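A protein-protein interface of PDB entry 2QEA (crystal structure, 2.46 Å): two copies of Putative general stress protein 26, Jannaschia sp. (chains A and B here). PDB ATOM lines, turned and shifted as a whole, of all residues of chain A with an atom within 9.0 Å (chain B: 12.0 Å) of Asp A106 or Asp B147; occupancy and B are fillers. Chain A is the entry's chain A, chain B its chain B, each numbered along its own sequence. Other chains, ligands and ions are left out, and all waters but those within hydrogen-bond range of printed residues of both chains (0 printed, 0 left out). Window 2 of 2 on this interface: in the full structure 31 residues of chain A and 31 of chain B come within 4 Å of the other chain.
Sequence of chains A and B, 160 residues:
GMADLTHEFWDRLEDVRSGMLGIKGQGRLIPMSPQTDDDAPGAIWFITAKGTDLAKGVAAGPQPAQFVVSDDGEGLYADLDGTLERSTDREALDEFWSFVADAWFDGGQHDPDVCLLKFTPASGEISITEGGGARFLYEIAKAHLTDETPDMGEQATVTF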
ATOM      1  N   TRP A  97      -0.987  -6.307 -12.031  1.00  0.00           N
ATOM      2  CA  TRP A  97      -1.192  -7.023 -10.766  1.00  0.00           C
ATOM      3  C   TRP A  97      -1.400  -8.514 -11.072  1.00  0.00           C
ATOM      4  O   TRP A  97      -2.083  -8.855 -12.044  1.00  0.00           O
ATOM      5  CB  TRP A  97      -2.397  -6.457 -10.007  1.00  0.00           C
ATOM      6  CG  TRP A  97      -2.497  -6.935  -8.608  1.00  0.00           C
ATOM      7  CD1 TRP A  97      -3.298  -7.930  -8.142  1.00  0.00           C
ATOM      8  CD2 TRP A  97      -1.755  -6.449  -7.482  1.00  0.00           C
ATOM      9  NE1 TRP A  97      -3.116  -8.090  -6.793  1.00  0.00           N
ATOM     10  CE2 TRP A  97      -2.175  -7.196  -6.356  1.00  0.00           C
ATOM     11  CE3 TRP A  97      -0.784  -5.446  -7.309  1.00  0.00           C
ATOM     12  CZ2 TRP A  97      -1.649  -6.983  -5.067  1.00  0.00           C
ATOM     13  CZ3 TRP A  97      -0.258  -5.227  -6.020  1.00  0.00           C
ATOM     14  CH2 TRP A  97      -0.693  -6.001  -4.918  1.00  0.00           C
ATOM     15  N   VAL A 100       0.894 -13.601  -7.674  1.00  0.00           N
ATOM     16  CA  VAL A 100       2.131 -13.491  -6.882  1.00  0.00           C
ATOM     17  C   VAL A 100       2.058 -12.246  -5.986  1.00  0.00           C
ATOM     18  O   VAL A 100       2.383 -12.330  -4.800  1.00  0.00           O
ATOM     19  CB  VAL A 100       3.412 -13.451  -7.781  1.00  0.00           C
ATOM     20  CG1 VAL A 100       4.674 -13.253  -6.944  1.00  0.00           C
ATOM     21  CG2 VAL A 100       3.533 -14.729  -8.599  1.00  0.00           C
ATOM     22  N   ALA A 101       1.621 -11.115  -6.555  1.00  0.00           N
ATOM     23  CA  ALA A 101       1.438  -9.852  -5.804  1.00  0.00           C
ATOM     24  C   ALA A 101       0.446  -9.977  -4.631  1.00  0.00           C
ATOM     25  O   ALA A 101       0.618  -9.303  -3.617  1.00  0.00           O
ATOM     26  CB  ALA A 101       1.015  -8.714  -6.741  1.00  0.00           C
ATOM     27  N   ASP A 102      -0.582 -10.821  -4.782  1.00  0.00           N
ATOM     28  CA  ASP A 102      -1.544 -11.120  -3.694  1.00  0.00           C
ATOM     29  C   ASP A 102      -0.893 -11.830  -2.498  1.00  0.00           C
ATOM     30  O   ASP A 102      -1.328 -11.635  -1.361  1.00  0.00           O
ATOM     31  CB  ASP A 102      -2.729 -11.968  -4.196  1.00  0.00           C
ATOM     32  CG  ASP A 102      -3.733 -11.162  -4.995  1.00  0.00           C
ATOM     33  OD1 ASP A 102      -4.318 -10.217  -4.426  1.00  0.00           O
ATOM     34  OD2 ASP A 102      -3.972 -11.494  -6.173  1.00  0.00           O
ATOM     35  N   ALA A 103       0.119 -12.660  -2.765  1.00  0.00           N
ATOM     36  CA  ALA A 103       0.861 -13.380  -1.720  1.00  0.00           C
ATOM     37  C   ALA A 103       1.700 -12.426  -0.858  1.00  0.00           C
ATOM     38  O   ALA A 103       1.661 -12.509   0.373  1.00  0.00           O
ATOM     39  CB  ALA A 103       1.752 -14.461  -2.338  1.00  0.00           C
ATOM     40  N   TRP A 104       2.445 -11.532  -1.513  1.00  0.00           N
ATOM     41  CA  TRP A 104       3.284 -10.532  -0.823  1.00  0.00           C
ATOM     42  C   TRP A 104       2.488  -9.450  -0.077  1.00  0.00           C
ATOM     43  O   TRP A 104       2.883  -9.055   1.024  1.00  0.00           O
ATOM     44  CB  TRP A 104       4.279  -9.871  -1.796  1.00  0.00           C
ATOM     45  CG  TRP A 104       5.427 -10.756  -2.161  1.00  0.00           C
ATOM     46  CD1 TRP A 104       5.474 -11.677  -3.168  1.00  0.00           C
ATOM     47  CD2 TRP A 104       6.702 -10.803  -1.514  1.00  0.00           C
ATOM     48  NE1 TRP A 104       6.702 -12.299  -3.190  1.00  0.00           N
ATOM     49  CE2 TRP A 104       7.478 -11.781  -2.186  1.00  0.00           C
ATOM     50  CE3 TRP A 104       7.269 -10.111  -0.427  1.00  0.00           C
ATOM     51  CZ2 TRP A 104       8.802 -12.089  -1.805  1.00  0.00           C
ATOM     52  CZ3 TRP A 104       8.590 -10.415  -0.044  1.00  0.00           C
ATOM     53  CH2 TRP A 104       9.338 -11.398  -0.735  1.00  0.00           C
ATOM     54  N   PHE A 105       1.390  -8.985  -0.680  1.00  0.00           N
ATOM     55  CA  PHE A 105       0.528  -7.934  -0.112  1.00  0.00           C
ATOM     56  C   PHE A 105      -0.872  -8.499   0.170  1.00  0.00           C
ATOM     57  O   PHE A 105      -1.709  -8.589  -0.735  1.00  0.00           O
ATOM     58  CB  PHE A 105       0.482  -6.733  -1.064  1.00  0.00           C
ATOM     59  CG  PHE A 105       1.842  -6.185  -1.389  1.00  0.00           C
ATOM     60  CD1 PHE A 105       2.477  -5.303  -0.511  1.00  0.00           C
ATOM     61  CD2 PHE A 105       2.508  -6.573  -2.555  1.00  0.00           C
ATOM     62  CE1 PHE A 105       3.755  -4.800  -0.798  1.00  0.00           C
ATOM     63  CE2 PHE A 105       3.785  -6.080  -2.855  1.00  0.00           C
ATOM     64  CZ  PHE A 105       4.408  -5.193  -1.973  1.00  0.00           C
ATOM     65  N   ASP A 106      -1.102  -8.882   1.430  1.00  0.00           N
ATOM     66  CA  ASP A 106      -2.386  -9.479   1.880  1.00  0.00           C
ATOM     67  C   ASP A 106      -3.662  -8.641   1.658  1.00  0.00           C
ATOM     68  O   ASP A 106      -4.756  -9.211   1.575  1.00  0.00           O
ATOM     69  CB  ASP A 106      -2.309  -9.950   3.356  1.00  0.00           C
ATOM     70  CG  ASP A 106      -2.011  -8.817   4.346  1.00  0.00           C
ATOM     71  OD1 ASP A 106      -1.428  -7.784   3.946  1.00  0.00           O
ATOM     72  OD2 ASP A 106      -2.340  -8.979   5.539  1.00  0.00           O
ATOM     73  N   GLY A 107      -3.518  -7.314   1.556  1.00  0.00           N
ATOM     74  CA  GLY A 107      -4.639  -6.389   1.320  1.00  0.00           C
ATOM     75  C   GLY A 107      -4.944  -6.026  -0.130  1.00  0.00           C
ATOM     76  O   GLY A 107      -5.500  -4.952  -0.380  1.00  0.00           O
ATOM     77  N   GLY A 108      -4.595  -6.901  -1.080  1.00  0.00           N
ATOM     78  CA  GLY A 108      -4.828  -6.657  -2.511  1.00  0.00           C
ATOM     79  C   GLY A 108      -3.957  -5.549  -3.079  1.00  0.00           C
ATOM     80  O   GLY A 108      -2.913  -5.220  -2.504  1.00  0.00           O
ATOM     81  N   GLN A 109      -4.374  -4.988  -4.218  1.00  0.00           N
ATOM     82  CA  GLN A 109      -3.645  -3.869  -4.852  1.00  0.00           C
ATOM     83  C   GLN A 109      -3.817  -2.541  -4.097  1.00  0.00           C
ATOM     84  O   GLN A 109      -2.968  -1.653  -4.227  1.00  0.00           O
ATOM     85  CB  GLN A 109      -3.974  -3.736  -6.349  1.00  0.00           C
ATOM     86  CG  GLN A 109      -5.382  -3.287  -6.719  1.00  0.00           C
ATOM     87  CD  GLN A 109      -5.618  -3.316  -8.225  1.00  0.00           C
ATOM     88  OE1 GLN A 109      -5.981  -2.304  -8.825  1.00  0.00           O
ATOM     89  NE2 GLN A 109      -5.386  -4.471  -8.843  1.00  0.00           N
ATOM     90  N   HIS A 110      -4.902  -2.415  -3.323  1.00  0.00           N
ATOM     91  CA  HIS A 110      -5.160  -1.256  -2.461  1.00  0.00           C
ATOM     92  C   HIS A 110      -4.758  -1.660  -1.031  1.00  0.00           C
ATOM     93  O   HIS A 110      -5.605  -1.819  -0.143  1.00  0.00           O
ATOM     94  CB  HIS A 110      -6.627  -0.809  -2.556  1.00  0.00           C
ATOM     95  CG  HIS A 110      -7.035  -0.369  -3.930  1.00  0.00           C
ATOM     96  ND1 HIS A 110      -6.662   0.846  -4.464  1.00  0.00           N
ATOM     97  CD2 HIS A 110      -7.789  -0.978  -4.875  1.00  0.00           C
ATOM     98  CE1 HIS A 110      -7.162   0.963  -5.681  1.00  0.00           C
ATOM     99  NE2 HIS A 110      -7.852  -0.130  -5.954  1.00  0.00           N
ATOM    100  N   ASP A 111      -3.449  -1.857  -0.860  1.00  0.00           N
ATOM    101  CA  ASP A 111      -2.794  -2.226   0.405  1.00  0.00           C
ATOM    102  C   ASP A 111      -1.867  -1.040   0.746  1.00  0.00           C
ATOM    103  O   ASP A 111      -1.263  -0.473  -0.172  1.00  0.00           O
ATOM    104  CB  ASP A 111      -2.019  -3.541   0.189  1.00  0.00           C
ATOM    105  CG  ASP A 111      -1.284  -4.050   1.435  1.00  0.00           C
ATOM    106  OD1 ASP A 111      -0.343  -3.388   1.923  1.00  0.00           O
ATOM    107  OD2 ASP A 111      -1.604  -5.169   1.889  1.00  0.00           O
ATOM    108  N   PRO A 112      -1.751  -0.657   2.046  1.00  0.00           N
ATOM    109  CA  PRO A 112      -0.892   0.494   2.407  1.00  0.00           C
ATOM    110  C   PRO A 112       0.587   0.373   2.025  1.00  0.00           C
ATOM    111  O   PRO A 112       1.197   1.382   1.689  1.00  0.00           O
ATOM    112  CB  PRO A 112      -1.036   0.583   3.934  1.00  0.00           C
ATOM    113  CG  PRO A 112      -1.495  -0.760   4.354  1.00  0.00           C
ATOM    114  CD  PRO A 112      -2.381  -1.230   3.250  1.00  0.00           C
ATOM    115  N   ASP A 113       1.133  -0.844   2.068  1.00  0.00           N
ATOM    116  CA  ASP A 113       2.543  -1.095   1.728  1.00  0.00           C
ATOM    117  C   ASP A 113       2.847  -1.162   0.223  1.00  0.00           C
ATOM    118  O   ASP A 113       4.016  -1.080  -0.143  1.00  0.00           O
ATOM    119  CB  ASP A 113       3.045  -2.385   2.406  1.00  0.00           C
ATOM    120  CG  ASP A 113       2.934  -2.345   3.934  1.00  0.00           C
ATOM    121  OD1 ASP A 113       2.593  -1.285   4.509  1.00  0.00           O
ATOM    122  OD2 ASP A 113       3.187  -3.395   4.565  1.00  0.00           O
ATOM    123  N   VAL A 114       1.829  -1.312  -0.636  1.00  0.00           N
ATOM    124  CA  VAL A 114       2.038  -1.406  -2.097  1.00  0.00           C
ATOM    125  C   VAL A 114       2.580  -0.095  -2.685  1.00  0.00           C
ATOM    126  O   VAL A 114       2.140   0.988  -2.300  1.00  0.00           O
ATOM    127  CB  VAL A 114       0.747  -1.862  -2.850  1.00  0.00           C
ATOM    128  CG1 VAL A 114       0.887  -1.731  -4.370  1.00  0.00           C
ATOM    129  CG2 VAL A 114       0.428  -3.291  -2.501  1.00  0.00           C
ATOM    130  N   TYR B 138       3.681 -23.935  -2.174  1.00  0.00           N
ATOM    131  CA  TYR B 138       3.394 -23.979  -0.730  1.00  0.00           C
ATOM    132  C   TYR B 138       3.383 -22.581  -0.104  1.00  0.00           C
ATOM    133  O   TYR B 138       2.469 -22.266   0.664  1.00  0.00           O
ATOM    134  CB  TYR B 138       4.392 -24.885   0.013  1.00  0.00           C
ATOM    135  CG  TYR B 138       4.302 -24.808   1.529  1.00  0.00           C
ATOM    136  CD1 TYR B 138       3.273 -25.454   2.224  1.00  0.00           C
ATOM    137  CD2 TYR B 138       5.251 -24.082   2.272  1.00  0.00           C
ATOM    138  CE1 TYR B 138       3.185 -25.379   3.627  1.00  0.00           C
ATOM    139  CE2 TYR B 138       5.171 -24.000   3.672  1.00  0.00           C
ATOM    140  CZ  TYR B 138       4.140 -24.651   4.340  1.00  0.00           C
ATOM    141  OH  TYR B 138       4.064 -24.575   5.708  1.00  0.00           O
ATOM    142  N   GLU B 139       4.401 -21.775  -0.417  1.00  0.00           N
ATOM    143  CA  GLU B 139       4.516 -20.400   0.106  1.00  0.00           C
ATOM    144  C   GLU B 139       3.345 -19.484  -0.287  1.00  0.00           C
ATOM    145  O   GLU B 139       2.955 -18.621   0.504  1.00  0.00           O
ATOM    146  CB  GLU B 139       5.861 -19.755  -0.284  1.00  0.00           C
ATOM    147  CG  GLU B 139       7.111 -20.355   0.405  1.00  0.00           C
ATOM    148  CD  GLU B 139       7.162 -20.162   1.924  1.00  0.00           C
ATOM    149  OE1 GLU B 139       6.471 -19.275   2.470  1.00  0.00           O
ATOM    150  OE2 GLU B 139       7.913 -20.913   2.579  1.00  0.00           O
ATOM    151  N   ILE B 140       2.801 -19.674  -1.494  1.00  0.00           N
ATOM    152  CA  ILE B 140       1.614 -18.929  -1.960  1.00  0.00           C
ATOM    153  C   ILE B 140       0.359 -19.387  -1.204  1.00  0.00           C
ATOM    154  O   ILE B 140      -0.460 -18.550  -0.820  1.00  0.00           O
ATOM    155  CB  ILE B 140       1.436 -19.015  -3.503  1.00  0.00           C
ATOM    156  CG1 ILE B 140       2.525 -18.170  -4.175  1.00  0.00           C
ATOM    157  CG2 ILE B 140       0.043 -18.534  -3.946  1.00  0.00           C
ATOM    158  CD1 ILE B 140       2.469 -18.161  -5.675  1.00  0.00           C
ATOM    159  N   ALA B 141       0.219 -20.702  -1.009  1.00  0.00           N
ATOM    160  CA  ALA B 141      -0.888 -21.275  -0.217  1.00  0.00           C
ATOM    161  C   ALA B 141      -0.791 -20.815   1.248  1.00  0.00           C
ATOM    162  O   ALA B 141      -1.802 -20.455   1.850  1.00  0.00           O
ATOM    163  CB  ALA B 141      -0.884 -22.799  -0.300  1.00  0.00           C
ATOM    164  N   LYS B 142       0.432 -20.822   1.790  1.00  0.00           N
ATOM    165  CA  LYS B 142       0.728 -20.349   3.156  1.00  0.00           C
ATOM    166  C   LYS B 142       0.412 -18.857   3.330  1.00  0.00           C
ATOM    167  O   LYS B 142      -0.095 -18.464   4.380  1.00  0.00           O
ATOM    168  CB  LYS B 142       2.203 -20.609   3.516  1.00  0.00           C
ATOM    169  CG  LYS B 142       2.595 -20.289   4.967  1.00  0.00           C
ATOM    170  CD  LYS B 142       4.073 -20.544   5.219  1.00  0.00           C
ATOM    171  CE  LYS B 142       4.459 -20.162   6.642  1.00  0.00           C
ATOM    172  NZ  LYS B 142       5.903 -20.394   6.939  1.00  0.00           N
ATOM    173  N   ALA B 143       0.727 -18.048   2.309  1.00  0.00           N
ATOM    174  CA  ALA B 143       0.478 -16.588   2.312  1.00  0.00           C
ATOM    175  C   ALA B 143      -0.985 -16.213   2.563  1.00  0.00           C
ATOM    176  O   ALA B 143      -1.256 -15.237   3.263  1.00  0.00           O
ATOM    177  CB  ALA B 143       0.964 -15.952   1.011  1.00  0.00           C
ATOM    178  N   HIS B 144      -1.910 -16.989   1.995  1.00  0.00           N
ATOM    179  CA  HIS B 144      -3.350 -16.786   2.208  1.00  0.00           C
ATOM    180  C   HIS B 144      -3.811 -17.338   3.566  1.00  0.00           C
ATOM    181  O   HIS B 144      -4.712 -16.768   4.182  1.00  0.00           O
ATOM    182  CB  HIS B 144      -4.174 -17.367   1.051  1.00  0.00           C
ATOM    183  CG  HIS B 144      -3.852 -16.747  -0.274  1.00  0.00           C
ATOM    184  ND1 HIS B 144      -4.089 -15.415  -0.547  1.00  0.00           N
ATOM    185  CD2 HIS B 144      -3.306 -17.271  -1.397  1.00  0.00           C
ATOM    186  CE1 HIS B 144      -3.697 -15.146  -1.780  1.00  0.00           C
ATOM    187  NE2 HIS B 144      -3.220 -16.254  -2.318  1.00  0.00           N
ATOM    188  N   LEU B 145      -3.198 -18.436   4.022  1.00  0.00           N
ATOM    189  CA  LEU B 145      -3.500 -19.030   5.340  1.00  0.00           C
ATOM    190  C   LEU B 145      -2.982 -18.184   6.516  1.00  0.00           C
ATOM    191  O   LEU B 145      -3.670 -18.073   7.531  1.00  0.00           O
ATOM    192  CB  LEU B 145      -2.904 -20.447   5.461  1.00  0.00           C
ATOM    193  CG  LEU B 145      -3.457 -21.571   4.574  1.00  0.00           C
ATOM    194  CD1 LEU B 145      -2.491 -22.750   4.517  1.00  0.00           C
ATOM    195  CD2 LEU B 145      -4.824 -22.027   5.048  1.00  0.00           C
ATOM    196  N   THR B 146      -1.787 -17.596   6.369  1.00  0.00           N
ATOM    197  CA  THR B 146      -1.101 -16.852   7.446  1.00  0.00           C
ATOM    198  C   THR B 146      -0.993 -15.320   7.339  1.00  0.00           C
ATOM    199  O   THR B 146      -0.707 -14.675   8.350  1.00  0.00           O
ATOM    200  CB  THR B 146       0.352 -17.384   7.612  1.00  0.00           C
ATOM    201  OG1 THR B 146       1.108 -17.132   6.419  1.00  0.00           O
ATOM    202  CG2 THR B 146       0.353 -18.879   7.911  1.00  0.00           C
ATOM    203  N   ASP B 147      -1.205 -14.753   6.144  1.00  0.00           N
ATOM    204  CA  ASP B 147      -1.005 -13.303   5.871  1.00  0.00           C
ATOM    205  C   ASP B 147       0.459 -12.843   6.109  1.00  0.00           C
ATOM    206  O   ASP B 147       0.716 -11.684   6.461  1.00  0.00           O
ATOM    207  CB  ASP B 147      -2.032 -12.412   6.615  1.00  0.00           C
ATOM    208  CG  ASP B 147      -3.455 -12.587   6.103  1.00  0.00           C
ATOM    209  OD1 ASP B 147      -3.656 -12.748   4.878  1.00  0.00           O
ATOM    210  OD2 ASP B 147      -4.392 -12.510   6.924  1.00  0.00           O
ATOM    211  N   GLU B 148       1.398 -13.769   5.890  1.00  0.00           N
ATOM    212  CA  GLU B 148       2.834 -13.536   6.015  1.00  0.00           C
ATOM    213  C   GLU B 148       3.384 -13.482   4.602  1.00  0.00           C
ATOM    214  O   GLU B 148       2.890 -14.193   3.715  1.00  0.00           O
ATOM    215  CB  GLU B 148       3.515 -14.689   6.755  1.00  0.00           C
ATOM    216  CG  GLU B 148       3.096 -14.862   8.214  1.00  0.00           C
ATOM    217  CD  GLU B 148       3.753 -16.066   8.903  1.00  0.00           C
ATOM    218  OE1 GLU B 148       4.331 -16.945   8.220  1.00  0.00           O
ATOM    219  OE2 GLU B 148       3.683 -16.139  10.148  1.00  0.00           O
ATOM    220  N   THR B 149       4.405 -12.653   4.395  1.00  0.00           N
ATOM    221  CA  THR B 149       5.042 -12.529   3.085  1.00  0.00           C
ATOM    222  C   THR B 149       5.830 -13.824   2.796  1.00  0.00           C
ATOM    223  O   THR B 149       6.450 -14.364   3.720  1.00  0.00           O
ATOM    224  CB  THR B 149       5.985 -11.308   3.008  1.00  0.00           C
ATOM    225  OG1 THR B 149       6.958 -11.383   4.057  1.00  0.00           O
ATOM    226  CG2 THR B 149       5.198 -10.013   3.154  1.00  0.00           C
ATOM    227  N   PRO B 150       5.763 -14.356   1.549  1.00  0.00           N
ATOM    228  CA  PRO B 150       6.519 -15.562   1.186  1.00  0.00           C
ATOM    229  C   PRO B 150       8.032 -15.443   1.389  1.00  0.00           C
ATOM    230  O   PRO B 150       8.600 -14.383   1.098  1.00  0.00           O
ATOM    231  CB  PRO B 150       6.236 -15.707  -0.318  1.00  0.00           C
ATOM    232  CG  PRO B 150       4.957 -15.072  -0.519  1.00  0.00           C
ATOM    233  CD  PRO B 150       4.947 -13.899   0.406  1.00  0.00           C
ATOM    234  N   ASP B 151       8.651 -16.509   1.903  1.00  0.00           N
ATOM    235  CA  ASP B 151      10.098 -16.590   2.085  1.00  0.00           C
ATOM    236  C   ASP B 151      10.605 -17.572   1.023  1.00  0.00           C
ATOM    237  O   ASP B 151      10.600 -18.794   1.236  1.00  0.00           O
ATOM    238  CB  ASP B 151      10.457 -17.040   3.512  1.00  0.00           C
ATOM    239  CG  ASP B 151      11.971 -17.094   3.764  1.00  0.00           C
ATOM    240  OD1 ASP B 151      12.740 -16.330   3.138  1.00  0.00           O
ATOM    241  OD2 ASP B 151      12.393 -17.901   4.619  1.00  0.00           O
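Of the 14 printed residues of chain B, 5 touch a printed residue of chain A. Hydrophobic or aromatic side chains of chain B within 4 Å of the printed part of chain A: Ala B143 and Pro B150. Along chain B the printed residues that touch a printed residue of chain A span positions 143 to 150. Of the 16 printed residues of chain A, 3 touch a printed residue of chain B. Hydrophobic or aromatic side chains of chain A that line the printed part of chain B: Ala A103 and Trp A104. Among the printed residues, 6 pairs touch across the chains. Among the printed residues, no Asp or Glu carboxylate lies within 4 Å of a Lys or Arg side-chain nitrogen of the other chain.
CB of Ala B143 touches O of Ala A103 (3.6 Å). Ala A103 touches Glu B148. Pro B150 touches Ala A103. Trp A104 touches Thr B149 (O to CG2, 3.3 Å). Trp A104 touches Pro B150. Asp B147 touches Asp A106 (OD1 to CB, 3.5 Å).
No position is printed for both chains. Of the 6 pairs that touch across the chains among the printed residues, none has its exchanged pair printed and touching as well.
The side-chain hydroxyl (OG1) of Thr B146 sits close to the backbone NH (N) of Glu B148 (3.4 Å).
Ala A103 touches just these residues of chain B: Ala B143, Glu B148 and Pro B150. Of the printed residues of chain B, Trp A104 touches Thr B149 (3.3 Å) and Pro B150 (3.6 Å). No residue of chain B comes within 4 Å of Phe A105. Asp A106 touches just one residue of chain B: Asp B147. No residue of chain B comes within 4 Å of Gly A108. Lys B142 touches none of the printed residues of chain A. No residue of chain A comes within 4 Å of Thr B146. Of chain A, only Asp A106 comes within 4 Å of Asp B147. Of the printed residues of chain A, Thr B149 touches Trp A104 (3.3 Å). Asp B151 touches none of the printed residues of chain A. The nearest residue of chain B that does not touch Asp A106 is Ala B143 (5.4 Å).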
